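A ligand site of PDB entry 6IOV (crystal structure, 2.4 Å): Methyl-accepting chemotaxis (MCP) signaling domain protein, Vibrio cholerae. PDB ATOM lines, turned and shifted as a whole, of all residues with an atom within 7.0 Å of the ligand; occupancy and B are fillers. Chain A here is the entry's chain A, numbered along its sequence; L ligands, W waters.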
ATOM      1  N   LEU A  70      -1.370 -16.782 -23.940  1.00  0.00           N
ATOM      2  CA  LEU A  70      -0.866 -16.835 -25.299  1.00  0.00           C
ATOM      3  C   LEU A  70      -1.925 -16.487 -26.333  1.00  0.00           C
ATOM      4  O   LEU A  70      -1.651 -15.860 -27.349  1.00  0.00           O
ATOM      5  CB  LEU A  70      -0.323 -18.222 -25.617  1.00  0.00           C
ATOM      6  CG  LEU A  70       1.055 -18.569 -25.113  1.00  0.00           C
ATOM      7  CD1 LEU A  70       1.404 -19.991 -25.523  1.00  0.00           C
ATOM      8  CD2 LEU A  70       2.020 -17.575 -25.723  1.00  0.00           C
ATOM      9  N   LEU A  71      -3.138 -16.945 -26.065  1.00  0.00           N
ATOM     10  CA  LEU A  71      -4.184 -16.992 -27.072  1.00  0.00           C
ATOM     11  C   LEU A  71      -5.484 -17.359 -26.375  1.00  0.00           C
ATOM     12  O   LEU A  71      -5.501 -18.181 -25.428  1.00  0.00           O
ATOM     13  CB  LEU A  71      -3.841 -18.028 -28.165  1.00  0.00           C
ATOM     14  CG  LEU A  71      -4.911 -18.164 -29.247  1.00  0.00           C
ATOM     15  CD1 LEU A  71      -5.072 -16.834 -29.968  1.00  0.00           C
ATOM     16  CD2 LEU A  71      -4.603 -19.278 -30.228  1.00  0.00           C
ATOM     17  N   ASN A  84     -11.552 -15.672 -31.719  1.00  0.00           N
ATOM     18  CA  ASN A  84     -10.314 -15.664 -30.956  1.00  0.00           C
ATOM     19  C   ASN A  84      -9.677 -14.254 -30.990  1.00  0.00           C
ATOM     20  O   ASN A  84     -10.085 -13.403 -31.768  1.00  0.00           O
ATOM     21  CB  ASN A  84      -9.356 -16.747 -31.477  1.00  0.00           C
ATOM     22  CG  ASN A  84      -8.827 -16.471 -32.891  1.00  0.00           C
ATOM     23  OD1 ASN A  84      -7.875 -15.718 -33.073  1.00  0.00           O
ATOM     24  ND2 ASN A  84      -9.438 -17.113 -33.888  1.00  0.00           N
ATOM     25  N   ASP A  86      -6.526 -13.417 -31.676  1.00  0.00           N
ATOM     26  CA  ASP A  86      -5.390 -13.264 -32.563  1.00  0.00           C
ATOM     27  C   ASP A  86      -5.872 -13.009 -34.006  1.00  0.00           C
ATOM     28  O   ASP A  86      -6.287 -13.927 -34.704  1.00  0.00           O
ATOM     29  CB  ASP A  86      -4.499 -14.501 -32.519  1.00  0.00           C
ATOM     30  CG  ASP A  86      -3.308 -14.403 -33.461  1.00  0.00           C
ATOM     31  OD1 ASP A  86      -3.059 -13.312 -34.013  1.00  0.00           O
ATOM     32  OD2 ASP A  86      -2.616 -15.425 -33.631  1.00  0.00           O
ATOM     33  N   TRP A  89      -4.708 -15.229 -36.851  1.00  0.00           N
ATOM     34  CA  TRP A  89      -5.072 -16.636 -36.841  1.00  0.00           C
ATOM     35  C   TRP A  89      -6.489 -16.843 -37.358  1.00  0.00           C
ATOM     36  O   TRP A  89      -7.477 -16.464 -36.716  1.00  0.00           O
ATOM     37  CB  TRP A  89      -4.930 -17.252 -35.442  1.00  0.00           C
ATOM     38  CG  TRP A  89      -5.150 -18.734 -35.453  1.00  0.00           C
ATOM     39  CD1 TRP A  89      -4.551 -19.645 -36.273  1.00  0.00           C
ATOM     40  CD2 TRP A  89      -6.045 -19.481 -34.608  1.00  0.00           C
ATOM     41  NE1 TRP A  89      -5.009 -20.912 -35.986  1.00  0.00           N
ATOM     42  CE2 TRP A  89      -5.929 -20.844 -34.972  1.00  0.00           C
ATOM     43  CE3 TRP A  89      -6.929 -19.134 -33.592  1.00  0.00           C
ATOM     44  CZ2 TRP A  89      -6.666 -21.850 -34.361  1.00  0.00           C
ATOM     45  CZ3 TRP A  89      -7.657 -20.132 -32.972  1.00  0.00           C
ATOM     46  CH2 TRP A  89      -7.523 -21.475 -33.362  1.00  0.00           C
ATOM     47  N   ASN A  90      -6.585 -17.417 -38.541  1.00  0.00           N
ATOM     48  CA  ASN A  90      -7.869 -17.678 -39.162  1.00  0.00           C
ATOM     49  C   ASN A  90      -7.895 -19.103 -39.648  1.00  0.00           C
ATOM     50  O   ASN A  90      -7.709 -19.361 -40.841  1.00  0.00           O
ATOM     51  CB  ASN A  90      -8.144 -16.710 -40.295  1.00  0.00           C
ATOM     52  CG  ASN A  90      -8.213 -15.297 -39.819  1.00  0.00           C
ATOM     53  OD1 ASN A  90      -9.206 -14.904 -39.196  1.00  0.00           O
ATOM     54  ND2 ASN A  90      -7.171 -14.521 -40.082  1.00  0.00           N
ATOM     55  N   PRO A  91      -8.099 -20.042 -38.709  1.00  0.00           N
ATOM     56  CA  PRO A  91      -8.109 -21.465 -39.053  1.00  0.00           C
ATOM     57  C   PRO A  91      -9.266 -21.723 -39.999  1.00  0.00           C
ATOM     58  O   PRO A  91     -10.350 -21.139 -39.834  1.00  0.00           O
ATOM     59  CB  PRO A  91      -8.306 -22.155 -37.702  1.00  0.00           C
ATOM     60  CG  PRO A  91      -9.145 -21.174 -36.927  1.00  0.00           C
ATOM     61  CD  PRO A  91      -8.563 -19.815 -37.324  1.00  0.00           C
ATOM     62  N   TRP A  95      -9.946 -27.141 -38.769  1.00  0.00           N
ATOM     63  CA  TRP A  95      -9.824 -26.938 -37.336  1.00  0.00           C
ATOM     64  C   TRP A  95     -11.208 -26.830 -36.714  1.00  0.00           C
ATOM     65  O   TRP A  95     -11.849 -25.791 -36.777  1.00  0.00           O
ATOM     66  CB  TRP A  95      -9.004 -25.686 -37.008  1.00  0.00           C
ATOM     67  CG  TRP A  95      -8.628 -25.625 -35.552  1.00  0.00           C
ATOM     68  CD1 TRP A  95      -7.638 -26.323 -34.928  1.00  0.00           C
ATOM     69  CD2 TRP A  95      -9.246 -24.826 -34.532  1.00  0.00           C
ATOM     70  NE1 TRP A  95      -7.599 -26.022 -33.584  1.00  0.00           N
ATOM     71  CE2 TRP A  95      -8.584 -25.109 -33.317  1.00  0.00           C
ATOM     72  CE3 TRP A  95     -10.297 -23.902 -34.527  1.00  0.00           C
ATOM     73  CZ2 TRP A  95      -8.939 -24.484 -32.106  1.00  0.00           C
ATOM     74  CZ3 TRP A  95     -10.648 -23.296 -33.340  1.00  0.00           C
ATOM     75  CH2 TRP A  95      -9.971 -23.578 -32.153  1.00  0.00           C
ATOM     76  N   PRO A  97     -13.075 -26.773 -33.323  1.00  0.00           N
ATOM     77  CA  PRO A  97     -12.738 -26.650 -31.896  1.00  0.00           C
ATOM     78  C   PRO A  97     -13.419 -27.716 -31.027  1.00  0.00           C
ATOM     79  O   PRO A  97     -12.902 -28.036 -29.968  1.00  0.00           O
ATOM     80  CB  PRO A  97     -13.233 -25.237 -31.531  1.00  0.00           C
ATOM     81  CG  PRO A  97     -14.316 -24.944 -32.586  1.00  0.00           C
ATOM     82  CD  PRO A  97     -13.842 -25.617 -33.844  1.00  0.00           C
ATOM     83  N   ARG A 100     -11.308 -30.667 -29.999  1.00  0.00           N
ATOM     84  CA  ARG A 100     -10.051 -30.400 -29.292  1.00  0.00           C
ATOM     85  C   ARG A 100     -10.129 -30.809 -27.816  1.00  0.00           C
ATOM     86  O   ARG A 100     -11.199 -30.789 -27.215  1.00  0.00           O
ATOM     87  CB  ARG A 100      -9.660 -28.923 -29.422  1.00  0.00           C
ATOM     88  CG  ARG A 100      -9.392 -28.463 -30.854  1.00  0.00           C
ATOM     89  CD  ARG A 100      -8.235 -29.211 -31.500  1.00  0.00           C
ATOM     90  NE  ARG A 100      -6.935 -28.820 -30.971  1.00  0.00           N
ATOM     91  CZ  ARG A 100      -5.884 -29.633 -30.870  1.00  0.00           C
ATOM     92  NH1 ARG A 100      -5.976 -30.912 -31.263  1.00  0.00           N
ATOM     93  NH2 ARG A 100      -4.746 -29.186 -30.380  1.00  0.00           N
ATOM     94  N   PRO A 101      -8.993 -31.222 -27.236  1.00  0.00           N
ATOM     95  CA  PRO A 101      -8.915 -31.642 -25.831  1.00  0.00           C
ATOM     96  C   PRO A 101      -9.432 -30.603 -24.839  1.00  0.00           C
ATOM     97  O   PRO A 101     -10.148 -30.975 -23.900  1.00  0.00           O
ATOM     98  CB  PRO A 101      -7.413 -31.889 -25.605  1.00  0.00           C
ATOM     99  CG  PRO A 101      -6.707 -31.329 -26.836  1.00  0.00           C
ATOM    100  CD  PRO A 101      -7.706 -31.424 -27.947  1.00  0.00           C
ATOM    101  N   TRP A 102      -9.066 -29.332 -25.006  1.00  0.00           N
ATOM    102  CA  TRP A 102      -9.531 -28.284 -24.091  1.00  0.00           C
ATOM    103  C   TRP A 102     -11.050 -28.137 -24.129  1.00  0.00           C
ATOM    104  O   TRP A 102     -11.697 -27.949 -23.091  1.00  0.00           O
ATOM    105  CB  TRP A 102      -8.858 -26.941 -24.410  1.00  0.00           C
ATOM    106  CG  TRP A 102      -8.976 -26.510 -25.843  1.00  0.00           C
ATOM    107  CD1 TRP A 102      -8.050 -26.704 -26.842  1.00  0.00           C
ATOM    108  CD2 TRP A 102     -10.069 -25.787 -26.431  1.00  0.00           C
ATOM    109  NE1 TRP A 102      -8.518 -26.154 -28.025  1.00  0.00           N
ATOM    110  CE2 TRP A 102      -9.749 -25.590 -27.792  1.00  0.00           C
ATOM    111  CE3 TRP A 102     -11.288 -25.286 -25.942  1.00  0.00           C
ATOM    112  CZ2 TRP A 102     -10.611 -24.928 -28.682  1.00  0.00           C
ATOM    113  CZ3 TRP A 102     -12.150 -24.625 -26.818  1.00  0.00           C
ATOM    114  CH2 TRP A 102     -11.804 -24.443 -28.181  1.00  0.00           C
ATOM    115  N   TYR A 118      -0.659 -30.858 -23.970  1.00  0.00           N
ATOM    116  CA  TYR A 118      -1.015 -31.390 -25.271  1.00  0.00           C
ATOM    117  C   TYR A 118      -0.356 -30.551 -26.358  1.00  0.00           C
ATOM    118  O   TYR A 118       0.170 -29.485 -26.069  1.00  0.00           O
ATOM    119  CB  TYR A 118      -2.545 -31.449 -25.460  1.00  0.00           C
ATOM    120  CG  TYR A 118      -3.183 -30.083 -25.615  1.00  0.00           C
ATOM    121  CD1 TYR A 118      -3.476 -29.316 -24.494  1.00  0.00           C
ATOM    122  CD2 TYR A 118      -3.478 -29.567 -26.877  1.00  0.00           C
ATOM    123  CE1 TYR A 118      -4.040 -28.060 -24.610  1.00  0.00           C
ATOM    124  CE2 TYR A 118      -4.048 -28.297 -27.013  1.00  0.00           C
ATOM    125  CZ  TYR A 118      -4.336 -27.543 -25.873  1.00  0.00           C
ATOM    126  OH  TYR A 118      -4.887 -26.293 -25.961  1.00  0.00           O
ATOM    127  N   ALA A 119      -0.343 -31.038 -27.593  1.00  0.00           N
ATOM    128  CA  ALA A 119       0.292 -30.325 -28.694  1.00  0.00           C
ATOM    129  C   ALA A 119      -0.633 -29.281 -29.322  1.00  0.00           C
ATOM    130  O   ALA A 119      -1.725 -29.599 -29.762  1.00  0.00           O
ATOM    131  CB  ALA A 119       0.780 -31.318 -29.774  1.00  0.00           C
ATOM    132  N   ASP A 120      -0.184 -28.032 -29.348  1.00  0.00           N
ATOM    133  CA  ASP A 120      -0.906 -26.942 -29.990  1.00  0.00           C
ATOM    134  C   ASP A 120      -1.158 -27.185 -31.493  1.00  0.00           C
ATOM    135  O   ASP A 120      -0.273 -27.648 -32.217  1.00  0.00           O
ATOM    136  CB  ASP A 120      -0.142 -25.634 -29.792  1.00  0.00           C
ATOM    137  CG  ASP A 120      -0.831 -24.445 -30.465  1.00  0.00           C
ATOM    138  OD1 ASP A 120      -1.695 -23.824 -29.816  1.00  0.00           O
ATOM    139  OD2 ASP A 120      -0.502 -24.169 -31.640  1.00  0.00           O
ATOM    140  N   SER A 121      -2.351 -26.845 -31.968  1.00  0.00           N
ATOM    141  CA  SER A 121      -2.747 -27.051 -33.376  1.00  0.00           C
ATOM    142  C   SER A 121      -1.854 -26.346 -34.389  1.00  0.00           C
ATOM    143  O   SER A 121      -1.533 -26.892 -35.428  1.00  0.00           O
ATOM    144  CB  SER A 121      -4.182 -26.558 -33.623  1.00  0.00           C
ATOM    145  OG  SER A 121      -5.107 -27.452 -33.051  1.00  0.00           O
ATOM    146  N   ALA A 122      -1.497 -25.108 -34.069  1.00  0.00           N
ATOM    147  CA  ALA A 122      -0.725 -24.287 -35.000  1.00  0.00           C
ATOM    148  C   ALA A 122       0.764 -24.557 -34.912  1.00  0.00           C
ATOM    149  O   ALA A 122       1.408 -24.799 -35.920  1.00  0.00           O
ATOM    150  CB  ALA A 122      -1.023 -22.815 -34.754  1.00  0.00           C
ATOM    151  N   SER A 123       1.323 -24.513 -33.698  1.00  0.00           N
ATOM    152  CA  SER A 123       2.780 -24.612 -33.527  1.00  0.00           C
ATOM    153  C   SER A 123       3.295 -26.027 -33.280  1.00  0.00           C
ATOM    154  O   SER A 123       4.454 -26.319 -33.533  1.00  0.00           O
ATOM    155  CB  SER A 123       3.221 -23.732 -32.364  1.00  0.00           C
ATOM    156  OG  SER A 123       2.673 -24.179 -31.125  1.00  0.00           O
ATOM    157  N   GLU A 125       3.715 -26.989 -30.380  1.00  0.00           N
ATOM    158  CA  GLU A 125       4.333 -26.898 -29.053  1.00  0.00           C
ATOM    159  C   GLU A 125       3.415 -27.510 -28.001  1.00  0.00           C
ATOM    160  O   GLU A 125       2.180 -27.451 -28.102  1.00  0.00           O
ATOM    161  CB  GLU A 125       4.658 -25.447 -28.666  1.00  0.00           C
ATOM    162  CG  GLU A 125       5.598 -24.725 -29.635  1.00  0.00           C
ATOM    163  CD  GLU A 125       6.984 -24.499 -29.052  1.00  0.00           C
ATOM    164  OE1 GLU A 125       7.821 -25.443 -29.068  1.00  0.00           O
ATOM    165  OE2 GLU A 125       7.248 -23.375 -28.574  1.00  0.00           O
ATOM    166  N   LEU A 127       1.673 -27.280 -24.709  1.00  0.00           N
ATOM    167  CA  LEU A 127       1.212 -26.287 -23.772  1.00  0.00           C
ATOM    168  C   LEU A 127       0.127 -26.900 -22.886  1.00  0.00           C
ATOM    169  O   LEU A 127      -0.178 -28.099 -23.002  1.00  0.00           O
ATOM    170  CB  LEU A 127       0.695 -25.021 -24.505  1.00  0.00           C
ATOM    171  CG  LEU A 127      -0.272 -25.132 -25.711  1.00  0.00           C
ATOM    172  CD1 LEU A 127      -1.552 -25.764 -25.327  1.00  0.00           C
ATOM    173  CD2 LEU A 127      -0.575 -23.762 -26.366  1.00  0.00           C
ATOM    174  N   VAL A 128      -0.426 -26.090 -21.984  1.00  0.00           N
ATOM    175  CA  VAL A 128      -1.696 -26.408 -21.316  1.00  0.00           C
ATOM    176  C   VAL A 128      -2.638 -25.244 -21.533  1.00  0.00           C
ATOM    177  O   VAL A 128      -2.196 -24.134 -21.852  1.00  0.00           O
ATOM    178  CB  VAL A 128      -1.554 -26.680 -19.787  1.00  0.00           C
ATOM    179  CG1 VAL A 128      -0.616 -27.869 -19.531  1.00  0.00           C
ATOM    180  CG2 VAL A 128      -1.069 -25.433 -19.044  1.00  0.00           C
ATOM    181  N   SER A 129      -3.936 -25.500 -21.364  1.00  0.00           N
ATOM    182  CA  SER A 129      -4.946 -24.467 -21.482  1.00  0.00           C
ATOM    183  C   SER A 129      -5.875 -24.452 -20.261  1.00  0.00           C
ATOM    184  O   SER A 129      -6.334 -25.502 -19.807  1.00  0.00           O
ATOM    185  CB  SER A 129      -5.794 -24.674 -22.760  1.00  0.00           C
ATOM    186  OG  SER A 129      -4.998 -24.753 -23.926  1.00  0.00           O
ATOM    187  N   PHE A 147     -10.911 -21.455 -24.507  1.00  0.00           N
ATOM    188  CA  PHE A 147      -9.585 -21.849 -24.051  1.00  0.00           C
ATOM    189  C   PHE A 147      -8.718 -20.608 -23.788  1.00  0.00           C
ATOM    190  O   PHE A 147      -8.845 -19.566 -24.456  1.00  0.00           O
ATOM    191  CB  PHE A 147      -8.906 -22.785 -25.043  1.00  0.00           C
ATOM    192  CG  PHE A 147      -8.557 -22.130 -26.339  1.00  0.00           C
ATOM    193  CD1 PHE A 147      -7.345 -21.451 -26.483  1.00  0.00           C
ATOM    194  CD2 PHE A 147      -9.423 -22.173 -27.408  1.00  0.00           C
ATOM    195  CE1 PHE A 147      -7.013 -20.855 -27.679  1.00  0.00           C
ATOM    196  CE2 PHE A 147      -9.098 -21.575 -28.611  1.00  0.00           C
ATOM    197  CZ  PHE A 147      -7.888 -20.907 -28.742  1.00  0.00           C
ATOM    198  N   ASP A 149      -4.714 -20.101 -23.433  1.00  0.00           N
ATOM    199  CA  ASP A 149      -3.485 -20.871 -23.653  1.00  0.00           C
ATOM    200  C   ASP A 149      -2.389 -20.361 -22.743  1.00  0.00           C
ATOM    201  O   ASP A 149      -2.142 -19.157 -22.670  1.00  0.00           O
ATOM    202  CB  ASP A 149      -3.047 -20.806 -25.128  1.00  0.00           C
ATOM    203  CG  ASP A 149      -3.719 -21.862 -25.986  1.00  0.00           C
ATOM    204  OD1 ASP A 149      -4.423 -22.725 -25.422  1.00  0.00           O
ATOM    205  OD2 ASP A 149      -3.531 -21.838 -27.227  1.00  0.00           O
HETATM  206  N1  LIG L   1      -4.060 -24.229 -28.282  1.00  0.00           N
HETATM  207  C1  LIG L   1      -5.268 -24.342 -29.078  1.00  0.00           C
HETATM  208  C2  LIG L   1      -5.403 -25.728 -29.718  1.00  0.00           C
HETATM  209  O1  LIG L   1      -6.520 -26.146 -30.049  1.00  0.00           O
HETATM  210  C3  LIG L   1      -5.306 -23.268 -30.169  1.00  0.00           C
HETATM  211  C4  LIG L   1      -4.619 -23.691 -31.460  1.00  0.00           C
HETATM  212  C5  LIG L   1      -4.177 -22.485 -32.266  1.00  0.00           C
HETATM  213  N2  LIG L   1      -2.986 -21.870 -31.720  1.00  0.00           N
HETATM  214  C6  LIG L   1      -2.428 -20.754 -32.194  1.00  0.00           C
HETATM  215  N3  LIG L   1      -1.333 -20.267 -31.621  1.00  0.00           N
HETATM  216  N4  LIG L   1      -2.979 -20.113 -33.225  1.00  0.00           N
HETATM  217  O2  LIG L   1      -4.425 -26.452 -29.922  1.00  0.00           O
HETATM  218  O   HOH W   1      -1.220 -21.231 -28.461  1.00  0.00           O
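Leu 71 touches the ligand. Trp 89 touches the ligand (CZ2 to C5, 3.3 Å). Trp 95 touches the ligand (CZ2 to O1, 3.6 Å). CB of Ala 122 touches C6 of the ligand (3.6 Å). Phe 147 touches the ligand (CZ to C3, 3.8 Å). Hydrophobic or aromatic side chains that line the ligand: Leu 71, Trp 89, Trp 95, Trp 102, Tyr 118, Ala 122 and Phe 147. Within 4 Å of the ligand: Leu 71, Trp 89, Trp 95, Arg 100, Trp 102, Tyr 118, Asp 120, Ser 121, Ala 122, Phe 147 and Asp 149. The nearest printed residue that does not touch the ligand is Leu 127 (4.004 Å).
Water W1 lies within hydrogen-bond range of OD2 of Asp 149 (2.7 Å), OD1 of Asp 120 (3.0 Å) and N3 of the ligand (3.3 Å).
OG of Ser 121 is in hydrogen-bond range of NE of Arg 100 (3.1 Å). The guanidinium group of Arg 100 lies within hydrogen-bond range of the backbone carbonyl oxygen of Ala 119 (3.1 Å). The indole nitrogen of Trp 95 is in hydrogen-bond range of the side-chain hydroxyl of Ser 121 (2.9 Å). The side-chain hydroxyl (OH) of Tyr 118 lies within hydrogen-bond range of the side-chain hydroxyl (OG) of Ser 129 (2.6 Å). N of Ser 123 is in hydrogen-bond range of OD2 of Asp 120. O of Asp 149 sits at hydrogen-bond distance from N of Leu 70 (2.8 Å). N of Asp 149 lies within hydrogen-bond range of O of Leu 71, at 2.9 Å. The side-chain carboxylate of Asp 120 lies within hydrogen-bond range of the backbone NH of Ala 122 (2.8 Å).
The side-chain hydroxyl (OH) of Tyr 118 sits at hydrogen-bond distance from a nitrogen (N1) of the ligand (3.2 Å). NE1 of Trp 102 is in hydrogen-bond range of O1 of the ligand (2.8 Å). NH2 of Arg 100 lies within salt-bridge range of O2 of the ligand, at 2.8 Å. The side-chain hydroxyl of Ser 121 is in hydrogen-bond range of an oxygen (O2) of the ligand (3.4 Å). N of Ser 121 is in hydrogen-bond range of O2 of the ligand (2.9 Å). The side-chain carboxylate (OD2) of Asp 149 lies within salt-bridge range of a nitrogen (N1) of the ligand, 2.7 Å away. OD1 of Asp 120 is in salt-bridge range of N1 of the ligand (2.8 Å).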
